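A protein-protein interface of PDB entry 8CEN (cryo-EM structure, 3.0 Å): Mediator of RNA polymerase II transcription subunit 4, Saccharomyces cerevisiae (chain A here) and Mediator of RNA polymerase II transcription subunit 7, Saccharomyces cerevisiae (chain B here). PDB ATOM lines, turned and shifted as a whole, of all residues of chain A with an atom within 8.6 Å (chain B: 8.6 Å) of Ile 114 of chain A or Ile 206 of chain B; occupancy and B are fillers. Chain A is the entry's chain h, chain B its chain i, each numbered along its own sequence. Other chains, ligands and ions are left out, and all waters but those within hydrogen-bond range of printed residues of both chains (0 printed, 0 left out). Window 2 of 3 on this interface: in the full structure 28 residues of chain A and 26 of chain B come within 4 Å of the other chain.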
ATOM      1  N   LEU A 107     -20.644   2.210 -27.067  1.00  0.00           N
ATOM      2  CA  LEU A 107     -21.674   1.607 -26.224  1.00  0.00           C
ATOM      3  C   LEU A 107     -22.850   1.112 -27.058  1.00  0.00           C
ATOM      4  O   LEU A 107     -23.445   0.080 -26.731  1.00  0.00           O
ATOM      5  CB  LEU A 107     -22.131   2.580 -25.128  1.00  0.00           C
ATOM      6  CG  LEU A 107     -22.987   3.836 -25.341  1.00  0.00           C
ATOM      7  CD1 LEU A 107     -24.484   3.544 -25.266  1.00  0.00           C
ATOM      8  CD2 LEU A 107     -22.612   4.900 -24.320  1.00  0.00           C
ATOM      9  N   ASP A 108     -23.182   1.813 -28.149  1.00  0.00           N
ATOM     10  CA  ASP A 108     -24.197   1.305 -29.070  1.00  0.00           C
ATOM     11  C   ASP A 108     -23.746   0.003 -29.729  1.00  0.00           C
ATOM     12  O   ASP A 108     -24.546  -0.930 -29.900  1.00  0.00           O
ATOM     13  CB  ASP A 108     -24.524   2.363 -30.124  1.00  0.00           C
ATOM     14  CG  ASP A 108     -25.502   3.405 -29.618  1.00  0.00           C
ATOM     15  OD1 ASP A 108     -26.135   3.167 -28.567  1.00  0.00           O
ATOM     16  OD2 ASP A 108     -25.638   4.463 -30.268  1.00  0.00           O
ATOM     17  N   SER A 109     -22.463  -0.077 -30.099  1.00  0.00           N
ATOM     18  CA  SER A 109     -21.911  -1.312 -30.648  1.00  0.00           C
ATOM     19  C   SER A 109     -21.956  -2.441 -29.625  1.00  0.00           C
ATOM     20  O   SER A 109     -22.264  -3.589 -29.970  1.00  0.00           O
ATOM     21  CB  SER A 109     -20.479  -1.077 -31.127  1.00  0.00           C
ATOM     22  OG  SER A 109     -20.425  -0.015 -32.063  1.00  0.00           O
ATOM     23  N   LYS A 110     -21.654  -2.128 -28.361  1.00  0.00           N
ATOM     24  CA  LYS A 110     -21.741  -3.120 -27.293  1.00  0.00           C
ATOM     25  C   LYS A 110     -23.166  -3.630 -27.126  1.00  0.00           C
ATOM     26  O   LYS A 110     -23.384  -4.839 -26.983  1.00  0.00           O
ATOM     27  CB  LYS A 110     -21.234  -2.522 -25.980  1.00  0.00           C
ATOM     28  CG  LYS A 110     -21.291  -3.476 -24.795  1.00  0.00           C
ATOM     29  CD  LYS A 110     -20.793  -2.812 -23.521  1.00  0.00           C
ATOM     30  CE  LYS A 110     -19.277  -2.822 -23.444  1.00  0.00           C
ATOM     31  NZ  LYS A 110     -18.756  -4.165 -23.072  1.00  0.00           N
ATOM     32  N   THR A 111     -24.149  -2.722 -27.154  1.00  0.00           N
ATOM     33  CA  THR A 111     -25.544  -3.132 -27.019  1.00  0.00           C
ATOM     34  C   THR A 111     -25.987  -4.018 -28.176  1.00  0.00           C
ATOM     35  O   THR A 111     -26.644  -5.042 -27.959  1.00  0.00           O
ATOM     36  CB  THR A 111     -26.463  -1.913 -26.910  1.00  0.00           C
ATOM     37  OG1 THR A 111     -26.264  -1.052 -28.038  1.00  0.00           O
ATOM     38  CG2 THR A 111     -26.217  -1.157 -25.612  1.00  0.00           C
ATOM     39  N   ARG A 112     -25.619  -3.662 -29.411  1.00  0.00           N
ATOM     40  CA  ARG A 112     -26.070  -4.483 -30.532  1.00  0.00           C
ATOM     41  C   ARG A 112     -25.358  -5.834 -30.570  1.00  0.00           C
ATOM     42  O   ARG A 112     -25.982  -6.847 -30.921  1.00  0.00           O
ATOM     43  CB  ARG A 112     -25.923  -3.730 -31.859  1.00  0.00           C
ATOM     44  CG  ARG A 112     -24.521  -3.330 -32.266  1.00  0.00           C
ATOM     45  CD  ARG A 112     -24.531  -2.646 -33.627  1.00  0.00           C
ATOM     46  NE  ARG A 112     -25.458  -1.519 -33.662  1.00  0.00           N
ATOM     47  CZ  ARG A 112     -25.129  -0.266 -33.382  1.00  0.00           C
ATOM     48  NH1 ARG A 112     -23.891   0.068 -33.053  1.00  0.00           N
ATOM     49  NH2 ARG A 112     -26.064   0.679 -33.439  1.00  0.00           N
ATOM     50  N   LYS A 113     -24.084  -5.895 -30.158  1.00  0.00           N
ATOM     51  CA  LYS A 113     -23.407  -7.190 -30.162  1.00  0.00           C
ATOM     52  C   LYS A 113     -23.915  -8.088 -29.036  1.00  0.00           C
ATOM     53  O   LYS A 113     -24.082  -9.297 -29.240  1.00  0.00           O
ATOM     54  CB  LYS A 113     -21.881  -7.012 -30.110  1.00  0.00           C
ATOM     55  CG  LYS A 113     -21.269  -6.445 -28.833  1.00  0.00           C
ATOM     56  CD  LYS A 113     -20.728  -7.530 -27.907  1.00  0.00           C
ATOM     57  CE  LYS A 113     -20.074  -6.928 -26.674  1.00  0.00           C
ATOM     58  NZ  LYS A 113     -19.591  -7.977 -25.733  1.00  0.00           N
ATOM     59  N   ILE A 114     -24.199  -7.526 -27.853  1.00  0.00           N
ATOM     60  CA  ILE A 114     -24.743  -8.370 -26.793  1.00  0.00           C
ATOM     61  C   ILE A 114     -26.169  -8.794 -27.148  1.00  0.00           C
ATOM     62  O   ILE A 114     -26.581  -9.927 -26.855  1.00  0.00           O
ATOM     63  CB  ILE A 114     -24.640  -7.680 -25.412  1.00  0.00           C
ATOM     64  CG1 ILE A 114     -24.961  -8.665 -24.290  1.00  0.00           C
ATOM     65  CG2 ILE A 114     -25.572  -6.495 -25.281  1.00  0.00           C
ATOM     66  CD1 ILE A 114     -24.585  -8.180 -22.916  1.00  0.00           C
ATOM     67  N   LEU A 115     -26.907  -7.940 -27.868  1.00  0.00           N
ATOM     68  CA  LEU A 115     -28.250  -8.300 -28.294  1.00  0.00           C
ATOM     69  C   LEU A 115     -28.221  -9.456 -29.284  1.00  0.00           C
ATOM     70  O   LEU A 115     -29.004 -10.406 -29.161  1.00  0.00           O
ATOM     71  CB  LEU A 115     -28.941  -7.088 -28.917  1.00  0.00           C
ATOM     72  CG  LEU A 115     -30.430  -7.275 -29.165  1.00  0.00           C
ATOM     73  CD1 LEU A 115     -31.065  -7.428 -27.815  1.00  0.00           C
ATOM     74  CD2 LEU A 115     -31.019  -6.092 -29.897  1.00  0.00           C
ATOM     75  N   GLU A 116     -27.292  -9.423 -30.245  1.00  0.00           N
ATOM     76  CA  GLU A 116     -27.251 -10.510 -31.217  1.00  0.00           C
ATOM     77  C   GLU A 116     -26.676 -11.793 -30.618  1.00  0.00           C
ATOM     78  O   GLU A 116     -27.086 -12.891 -31.022  1.00  0.00           O
ATOM     79  CB  GLU A 116     -26.489 -10.085 -32.476  1.00  0.00           C
ATOM     80  CG  GLU A 116     -25.015  -9.768 -32.311  1.00  0.00           C
ATOM     81  CD  GLU A 116     -24.123 -10.940 -32.673  1.00  0.00           C
ATOM     82  OE1 GLU A 116     -24.602 -11.874 -33.351  1.00  0.00           O
ATOM     83  OE2 GLU A 116     -22.933 -10.919 -32.297  1.00  0.00           O
ATOM     84  N   ILE A 117     -25.760 -11.700 -29.644  1.00  0.00           N
ATOM     85  CA  ILE A 117     -25.255 -12.947 -29.067  1.00  0.00           C
ATOM     86  C   ILE A 117     -26.296 -13.598 -28.156  1.00  0.00           C
ATOM     87  O   ILE A 117     -26.382 -14.830 -28.106  1.00  0.00           O
ATOM     88  CB  ILE A 117     -23.899 -12.765 -28.347  1.00  0.00           C
ATOM     89  CG1 ILE A 117     -24.016 -11.879 -27.111  1.00  0.00           C
ATOM     90  CG2 ILE A 117     -22.827 -12.270 -29.316  1.00  0.00           C
ATOM     91  CD1 ILE A 117     -22.726 -11.735 -26.344  1.00  0.00           C
ATOM     92  N   LEU A 118     -27.127 -12.817 -27.450  1.00  0.00           N
ATOM     93  CA  LEU A 118     -28.238 -13.462 -26.746  1.00  0.00           C
ATOM     94  C   LEU A 118     -29.351 -13.904 -27.688  1.00  0.00           C
ATOM     95  O   LEU A 118     -30.077 -14.843 -27.356  1.00  0.00           O
ATOM     96  CB  LEU A 118     -28.798 -12.596 -25.614  1.00  0.00           C
ATOM     97  CG  LEU A 118     -28.009 -12.570 -24.294  1.00  0.00           C
ATOM     98  CD1 LEU A 118     -26.696 -11.830 -24.329  1.00  0.00           C
ATOM     99  CD2 LEU A 118     -28.895 -12.031 -23.172  1.00  0.00           C
ATOM    100  N   ASN A 119     -29.504 -13.272 -28.855  1.00  0.00           N
ATOM    101  CA  ASN A 119     -30.397 -13.828 -29.871  1.00  0.00           C
ATOM    102  C   ASN A 119     -29.931 -15.213 -30.317  1.00  0.00           C
ATOM    103  O   ASN A 119     -30.733 -16.158 -30.405  1.00  0.00           O
ATOM    104  CB  ASN A 119     -30.464 -12.887 -31.072  1.00  0.00           C
ATOM    105  CG  ASN A 119     -31.812 -12.902 -31.752  1.00  0.00           C
ATOM    106  OD1 ASN A 119     -32.543 -13.890 -31.690  1.00  0.00           O
ATOM    107  ND2 ASN A 119     -32.135 -11.814 -32.435  1.00  0.00           N
ATOM    108  N   GLU A 120     -28.629 -15.349 -30.587  1.00  0.00           N
ATOM    109  CA  GLU A 120     -28.075 -16.643 -30.974  1.00  0.00           C
ATOM    110  C   GLU A 120     -28.172 -17.651 -29.835  1.00  0.00           C
ATOM    111  O   GLU A 120     -28.502 -18.817 -30.064  1.00  0.00           O
ATOM    112  CB  GLU A 120     -26.626 -16.485 -31.431  1.00  0.00           C
ATOM    113  CG  GLU A 120     -26.478 -15.779 -32.769  1.00  0.00           C
ATOM    114  CD  GLU A 120     -27.015 -16.602 -33.924  1.00  0.00           C
ATOM    115  OE1 GLU A 120     -26.904 -17.846 -33.876  1.00  0.00           O
ATOM    116  OE2 GLU A 120     -27.552 -16.004 -34.881  1.00  0.00           O
ATOM    117  N   CYS A 121     -27.903 -17.213 -28.601  1.00  0.00           N
ATOM    118  CA  CYS A 121     -28.051 -18.080 -27.436  1.00  0.00           C
ATOM    119  C   CYS A 121     -29.490 -18.556 -27.283  1.00  0.00           C
ATOM    120  O   CYS A 121     -29.742 -19.744 -27.029  1.00  0.00           O
ATOM    121  CB  CYS A 121     -27.599 -17.329 -26.184  1.00  0.00           C
ATOM    122  SG  CYS A 121     -27.655 -18.279 -24.660  1.00  0.00           S
ATOM    123  N   VAL B 199     -25.146 -22.073 -22.317  1.00  0.00           N
ATOM    124  CA  VAL B 199     -25.931 -20.890 -21.969  1.00  0.00           C
ATOM    125  C   VAL B 199     -25.447 -20.285 -20.654  1.00  0.00           C
ATOM    126  O   VAL B 199     -25.304 -19.059 -20.539  1.00  0.00           O
ATOM    127  CB  VAL B 199     -27.430 -21.234 -21.936  1.00  0.00           C
ATOM    128  CG1 VAL B 199     -28.251 -20.045 -21.469  1.00  0.00           C
ATOM    129  CG2 VAL B 199     -27.872 -21.644 -23.318  1.00  0.00           C
ATOM    130  N   HIS B 200     -25.158 -21.129 -19.654  1.00  0.00           N
ATOM    131  CA  HIS B 200     -24.655 -20.620 -18.375  1.00  0.00           C
ATOM    132  C   HIS B 200     -23.312 -19.910 -18.526  1.00  0.00           C
ATOM    133  O   HIS B 200     -23.119 -18.819 -17.979  1.00  0.00           O
ATOM    134  CB  HIS B 200     -24.532 -21.722 -17.316  1.00  0.00           C
ATOM    135  CG  HIS B 200     -25.833 -22.328 -16.890  1.00  0.00           C
ATOM    136  ND1 HIS B 200     -26.715 -21.669 -16.059  1.00  0.00           N
ATOM    137  CD2 HIS B 200     -26.351 -23.566 -17.075  1.00  0.00           C
ATOM    138  CE1 HIS B 200     -27.752 -22.448 -15.813  1.00  0.00           C
ATOM    139  NE2 HIS B 200     -27.556 -23.605 -16.418  1.00  0.00           N
ATOM    140  N   ASP B 201     -22.368 -20.497 -19.267  1.00  0.00           N
ATOM    141  CA  ASP B 201     -21.069 -19.834 -19.334  1.00  0.00           C
ATOM    142  C   ASP B 201     -21.056 -18.661 -20.312  1.00  0.00           C
ATOM    143  O   ASP B 201     -20.258 -17.737 -20.131  1.00  0.00           O
ATOM    144  CB  ASP B 201     -19.931 -20.851 -19.593  1.00  0.00           C
ATOM    145  CG  ASP B 201     -19.872 -21.409 -21.024  1.00  0.00           C
ATOM    146  OD1 ASP B 201     -20.661 -21.053 -21.913  1.00  0.00           O
ATOM    147  OD2 ASP B 201     -18.981 -22.250 -21.257  1.00  0.00           O
ATOM    148  N   LYS B 202     -21.958 -18.629 -21.299  1.00  0.00           N
ATOM    149  CA  LYS B 202     -22.083 -17.430 -22.122  1.00  0.00           C
ATOM    150  C   LYS B 202     -22.751 -16.297 -21.345  1.00  0.00           C
ATOM    151  O   LYS B 202     -22.404 -15.122 -21.523  1.00  0.00           O
ATOM    152  CB  LYS B 202     -22.852 -17.752 -23.402  1.00  0.00           C
ATOM    153  CG  LYS B 202     -22.724 -16.699 -24.486  1.00  0.00           C
ATOM    154  CD  LYS B 202     -22.651 -17.335 -25.866  1.00  0.00           C
ATOM    155  CE  LYS B 202     -23.979 -17.942 -26.276  1.00  0.00           C
ATOM    156  NZ  LYS B 202     -23.935 -18.492 -27.661  1.00  0.00           N
ATOM    157  N   LEU B 203     -23.696 -16.632 -20.461  1.00  0.00           N
ATOM    158  CA  LEU B 203     -24.250 -15.630 -19.557  1.00  0.00           C
ATOM    159  C   LEU B 203     -23.207 -15.163 -18.546  1.00  0.00           C
ATOM    160  O   LEU B 203     -23.192 -13.989 -18.163  1.00  0.00           O
ATOM    161  CB  LEU B 203     -25.487 -16.197 -18.859  1.00  0.00           C
ATOM    162  CG  LEU B 203     -26.407 -15.276 -18.057  1.00  0.00           C
ATOM    163  CD1 LEU B 203     -27.853 -15.682 -18.282  1.00  0.00           C
ATOM    164  CD2 LEU B 203     -26.076 -15.336 -16.573  1.00  0.00           C
ATOM    165  N   THR B 204     -22.317 -16.060 -18.120  1.00  0.00           N
ATOM    166  CA  THR B 204     -21.193 -15.648 -17.288  1.00  0.00           C
ATOM    167  C   THR B 204     -20.255 -14.725 -18.058  1.00  0.00           C
ATOM    168  O   THR B 204     -19.699 -13.778 -17.492  1.00  0.00           O
ATOM    169  CB  THR B 204     -20.445 -16.880 -16.774  1.00  0.00           C
ATOM    170  OG1 THR B 204     -21.379 -17.789 -16.177  1.00  0.00           O
ATOM    171  CG2 THR B 204     -19.409 -16.489 -15.731  1.00  0.00           C
ATOM    172  N   SER B 205     -20.079 -14.978 -19.358  1.00  0.00           N
ATOM    173  CA  SER B 205     -19.239 -14.118 -20.188  1.00  0.00           C
ATOM    174  C   SER B 205     -19.840 -12.725 -20.348  1.00  0.00           C
ATOM    175  O   SER B 205     -19.116 -11.721 -20.277  1.00  0.00           O
ATOM    176  CB  SER B 205     -19.018 -14.762 -21.556  1.00  0.00           C
ATOM    177  OG  SER B 205     -20.169 -14.632 -22.372  1.00  0.00           O
ATOM    178  N   ILE B 206     -21.156 -12.636 -20.576  1.00  0.00           N
ATOM    179  CA  ILE B 206     -21.755 -11.306 -20.696  1.00  0.00           C
ATOM    180  C   ILE B 206     -21.764 -10.608 -19.339  1.00  0.00           C
ATOM    181  O   ILE B 206     -21.621  -9.383 -19.270  1.00  0.00           O
ATOM    182  CB  ILE B 206     -23.166 -11.334 -21.322  1.00  0.00           C
ATOM    183  CG1 ILE B 206     -24.170 -12.076 -20.446  1.00  0.00           C
ATOM    184  CG2 ILE B 206     -23.123 -11.968 -22.697  1.00  0.00           C
ATOM    185  CD1 ILE B 206     -25.603 -11.921 -20.865  1.00  0.00           C
ATOM    186  N   GLN B 207     -21.890 -11.368 -18.244  1.00  0.00           N
ATOM    187  CA  GLN B 207     -21.767 -10.789 -16.910  1.00  0.00           C
ATOM    188  C   GLN B 207     -20.365 -10.237 -16.670  1.00  0.00           C
ATOM    189  O   GLN B 207     -20.207  -9.147 -16.108  1.00  0.00           O
ATOM    190  CB  GLN B 207     -22.121 -11.845 -15.863  1.00  0.00           C
ATOM    191  CG  GLN B 207     -21.921 -11.416 -14.426  1.00  0.00           C
ATOM    192  CD  GLN B 207     -21.908 -12.596 -13.478  1.00  0.00           C
ATOM    193  OE1 GLN B 207     -22.613 -12.607 -12.470  1.00  0.00           O
ATOM    194  NE2 GLN B 207     -21.107 -13.605 -13.802  1.00  0.00           N
ATOM    195  N   ASP B 208     -19.338 -10.971 -17.106  1.00  0.00           N
ATOM    196  CA  ASP B 208     -17.961 -10.522 -16.924  1.00  0.00           C
ATOM    197  C   ASP B 208     -17.660  -9.286 -17.761  1.00  0.00           C
ATOM    198  O   ASP B 208     -17.009  -8.350 -17.280  1.00  0.00           O
ATOM    199  CB  ASP B 208     -16.992 -11.653 -17.267  1.00  0.00           C
ATOM    200  CG  ASP B 208     -16.960 -12.733 -16.204  1.00  0.00           C
ATOM    201  OD1 ASP B 208     -17.282 -12.428 -15.038  1.00  0.00           O
ATOM    202  OD2 ASP B 208     -16.614 -13.886 -16.535  1.00  0.00           O
ATOM    203  N   THR B 209     -18.130  -9.251 -19.012  1.00  0.00           N
ATOM    204  CA  THR B 209     -17.892  -8.058 -19.818  1.00  0.00           C
ATOM    205  C   THR B 209     -18.746  -6.877 -19.361  1.00  0.00           C
ATOM    206  O   THR B 209     -18.326  -5.728 -19.529  1.00  0.00           O
ATOM    207  CB  THR B 209     -18.100  -8.354 -21.313  1.00  0.00           C
ATOM    208  OG1 THR B 209     -17.520  -7.303 -22.095  1.00  0.00           O
ATOM    209  CG2 THR B 209     -19.570  -8.483 -21.676  1.00  0.00           C
ATOM    210  N   LEU B 210     -19.898  -7.128 -18.729  1.00  0.00           N
ATOM    211  CA  LEU B 210     -20.667  -6.043 -18.127  1.00  0.00           C
ATOM    212  C   LEU B 210     -19.964  -5.494 -16.891  1.00  0.00           C
ATOM    213  O   LEU B 210     -19.989  -4.282 -16.644  1.00  0.00           O
ATOM    214  CB  LEU B 210     -22.072  -6.538 -17.786  1.00  0.00           C
ATOM    215  CG  LEU B 210     -22.976  -5.676 -16.906  1.00  0.00           C
ATOM    216  CD1 LEU B 210     -23.221  -4.317 -17.541  1.00  0.00           C
ATOM    217  CD2 LEU B 210     -24.286  -6.398 -16.663  1.00  0.00           C
ATOM    218  N   ARG B 211     -19.342  -6.372 -16.099  1.00  0.00           N
ATOM    219  CA  ARG B 211     -18.519  -5.918 -14.981  1.00  0.00           C
ATOM    220  C   ARG B 211     -17.324  -5.109 -15.470  1.00  0.00           C
ATOM    221  O   ARG B 211     -16.942  -4.111 -14.846  1.00  0.00           O
ATOM    222  CB  ARG B 211     -18.036  -7.110 -14.155  1.00  0.00           C
ATOM    223  CG  ARG B 211     -19.105  -7.811 -13.337  1.00  0.00           C
ATOM    224  CD  ARG B 211     -18.687  -9.243 -13.039  1.00  0.00           C
ATOM    225  NE  ARG B 211     -19.528  -9.871 -12.027  1.00  0.00           N
ATOM    226  CZ  ARG B 211     -19.461 -11.151 -11.686  1.00  0.00           C
ATOM    227  NH1 ARG B 211     -18.600 -11.975 -12.261  1.00  0.00           N
ATOM    228  NH2 ARG B 211     -20.281 -11.617 -10.749  1.00  0.00           N
ATOM    229  N   THR B 212     -16.709  -5.541 -16.575  1.00  0.00           N
ATOM    230  CA  THR B 212     -15.580  -4.808 -17.142  1.00  0.00           C
ATOM    231  C   THR B 212     -16.006  -3.438 -17.659  1.00  0.00           C
ATOM    232  O   THR B 212     -15.301  -2.443 -17.453  1.00  0.00           O
ATOM    233  CB  THR B 212     -14.934  -5.627 -18.261  1.00  0.00           C
ATOM    234  OG1 THR B 212     -14.715  -6.968 -17.809  1.00  0.00           O
ATOM    235  CG2 THR B 212     -13.600  -5.015 -18.672  1.00  0.00           C
ATOM    236  N   GLY B 213     -17.158  -3.363 -18.325  1.00  0.00           N
ATOM    237  CA  GLY B 213     -17.660  -2.104 -18.834  1.00  0.00           C
ATOM    238  C   GLY B 213     -18.409  -1.241 -17.843  1.00  0.00           C
ATOM    239  O   GLY B 213     -18.794  -0.120 -18.185  1.00  0.00           O
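The side-chain hydroxyl (OG) of Ser 205 of chain B is in hydrogen-bond range of the backbone carbonyl oxygen (O) of Lys 202 of chain B (2.4 Å).
Among the printed residues, pairs that only touch across the chains: Lys 110 of chain A with Thr 209 of chain B, Ile 114 of chain A with Ile 206 of chain B, Ile 117 of chain A with Ile 206 of chain B, Leu 118 of chain A with Ile 206 of chain B, Cys 121 of chain A with Val 199 of chain B and Cys 121 of chain A with Lys 202 of chain B.
Of the 15 printed residues of chain B, 4 touch a printed residue of chain A.
Of the 15 printed residues of chain A, 5 touch a printed residue of chain B.
Printed residues of chain A that touch a printed residue of chain B: Lys 110, Ile 114, Ile 117, Leu 118 and Cys 121.
Among the printed residues, no Asp or Glu carboxylate lies within 4 Å of a Lys or Arg side-chain nitrogen of the other chain.
Of chain B, only Ile 206 comes within 4 Å of Ile 114 of chain A.
Glu 116 of chain A touches none of the printed residues of chain B.
Of the printed residues of chain B, Ile 117 of chain A touches Ile 206 (3.7 Å).
Printed residues of chain B within 4 Å of Leu 118 of chain A: Ile 206.
Glu 120 of chain A touches none of the printed residues of chain B.
Printed residues of chain A within 4 Å of Val 199 of chain B: Cys 121 (3.6 Å).
No residue of chain A comes within 4 Å of Ser 205 of chain B.
Of chain A, only Ile 114 (3.8 Å), Ile 117 (3.7 Å) and Leu 118 (3.6 Å) come within 4 Å of Ile 206 of chain B.
The nearest residue of chain A that does not touch Ile 206 of chain B is Lys 113 of chain A (6.1 Å).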
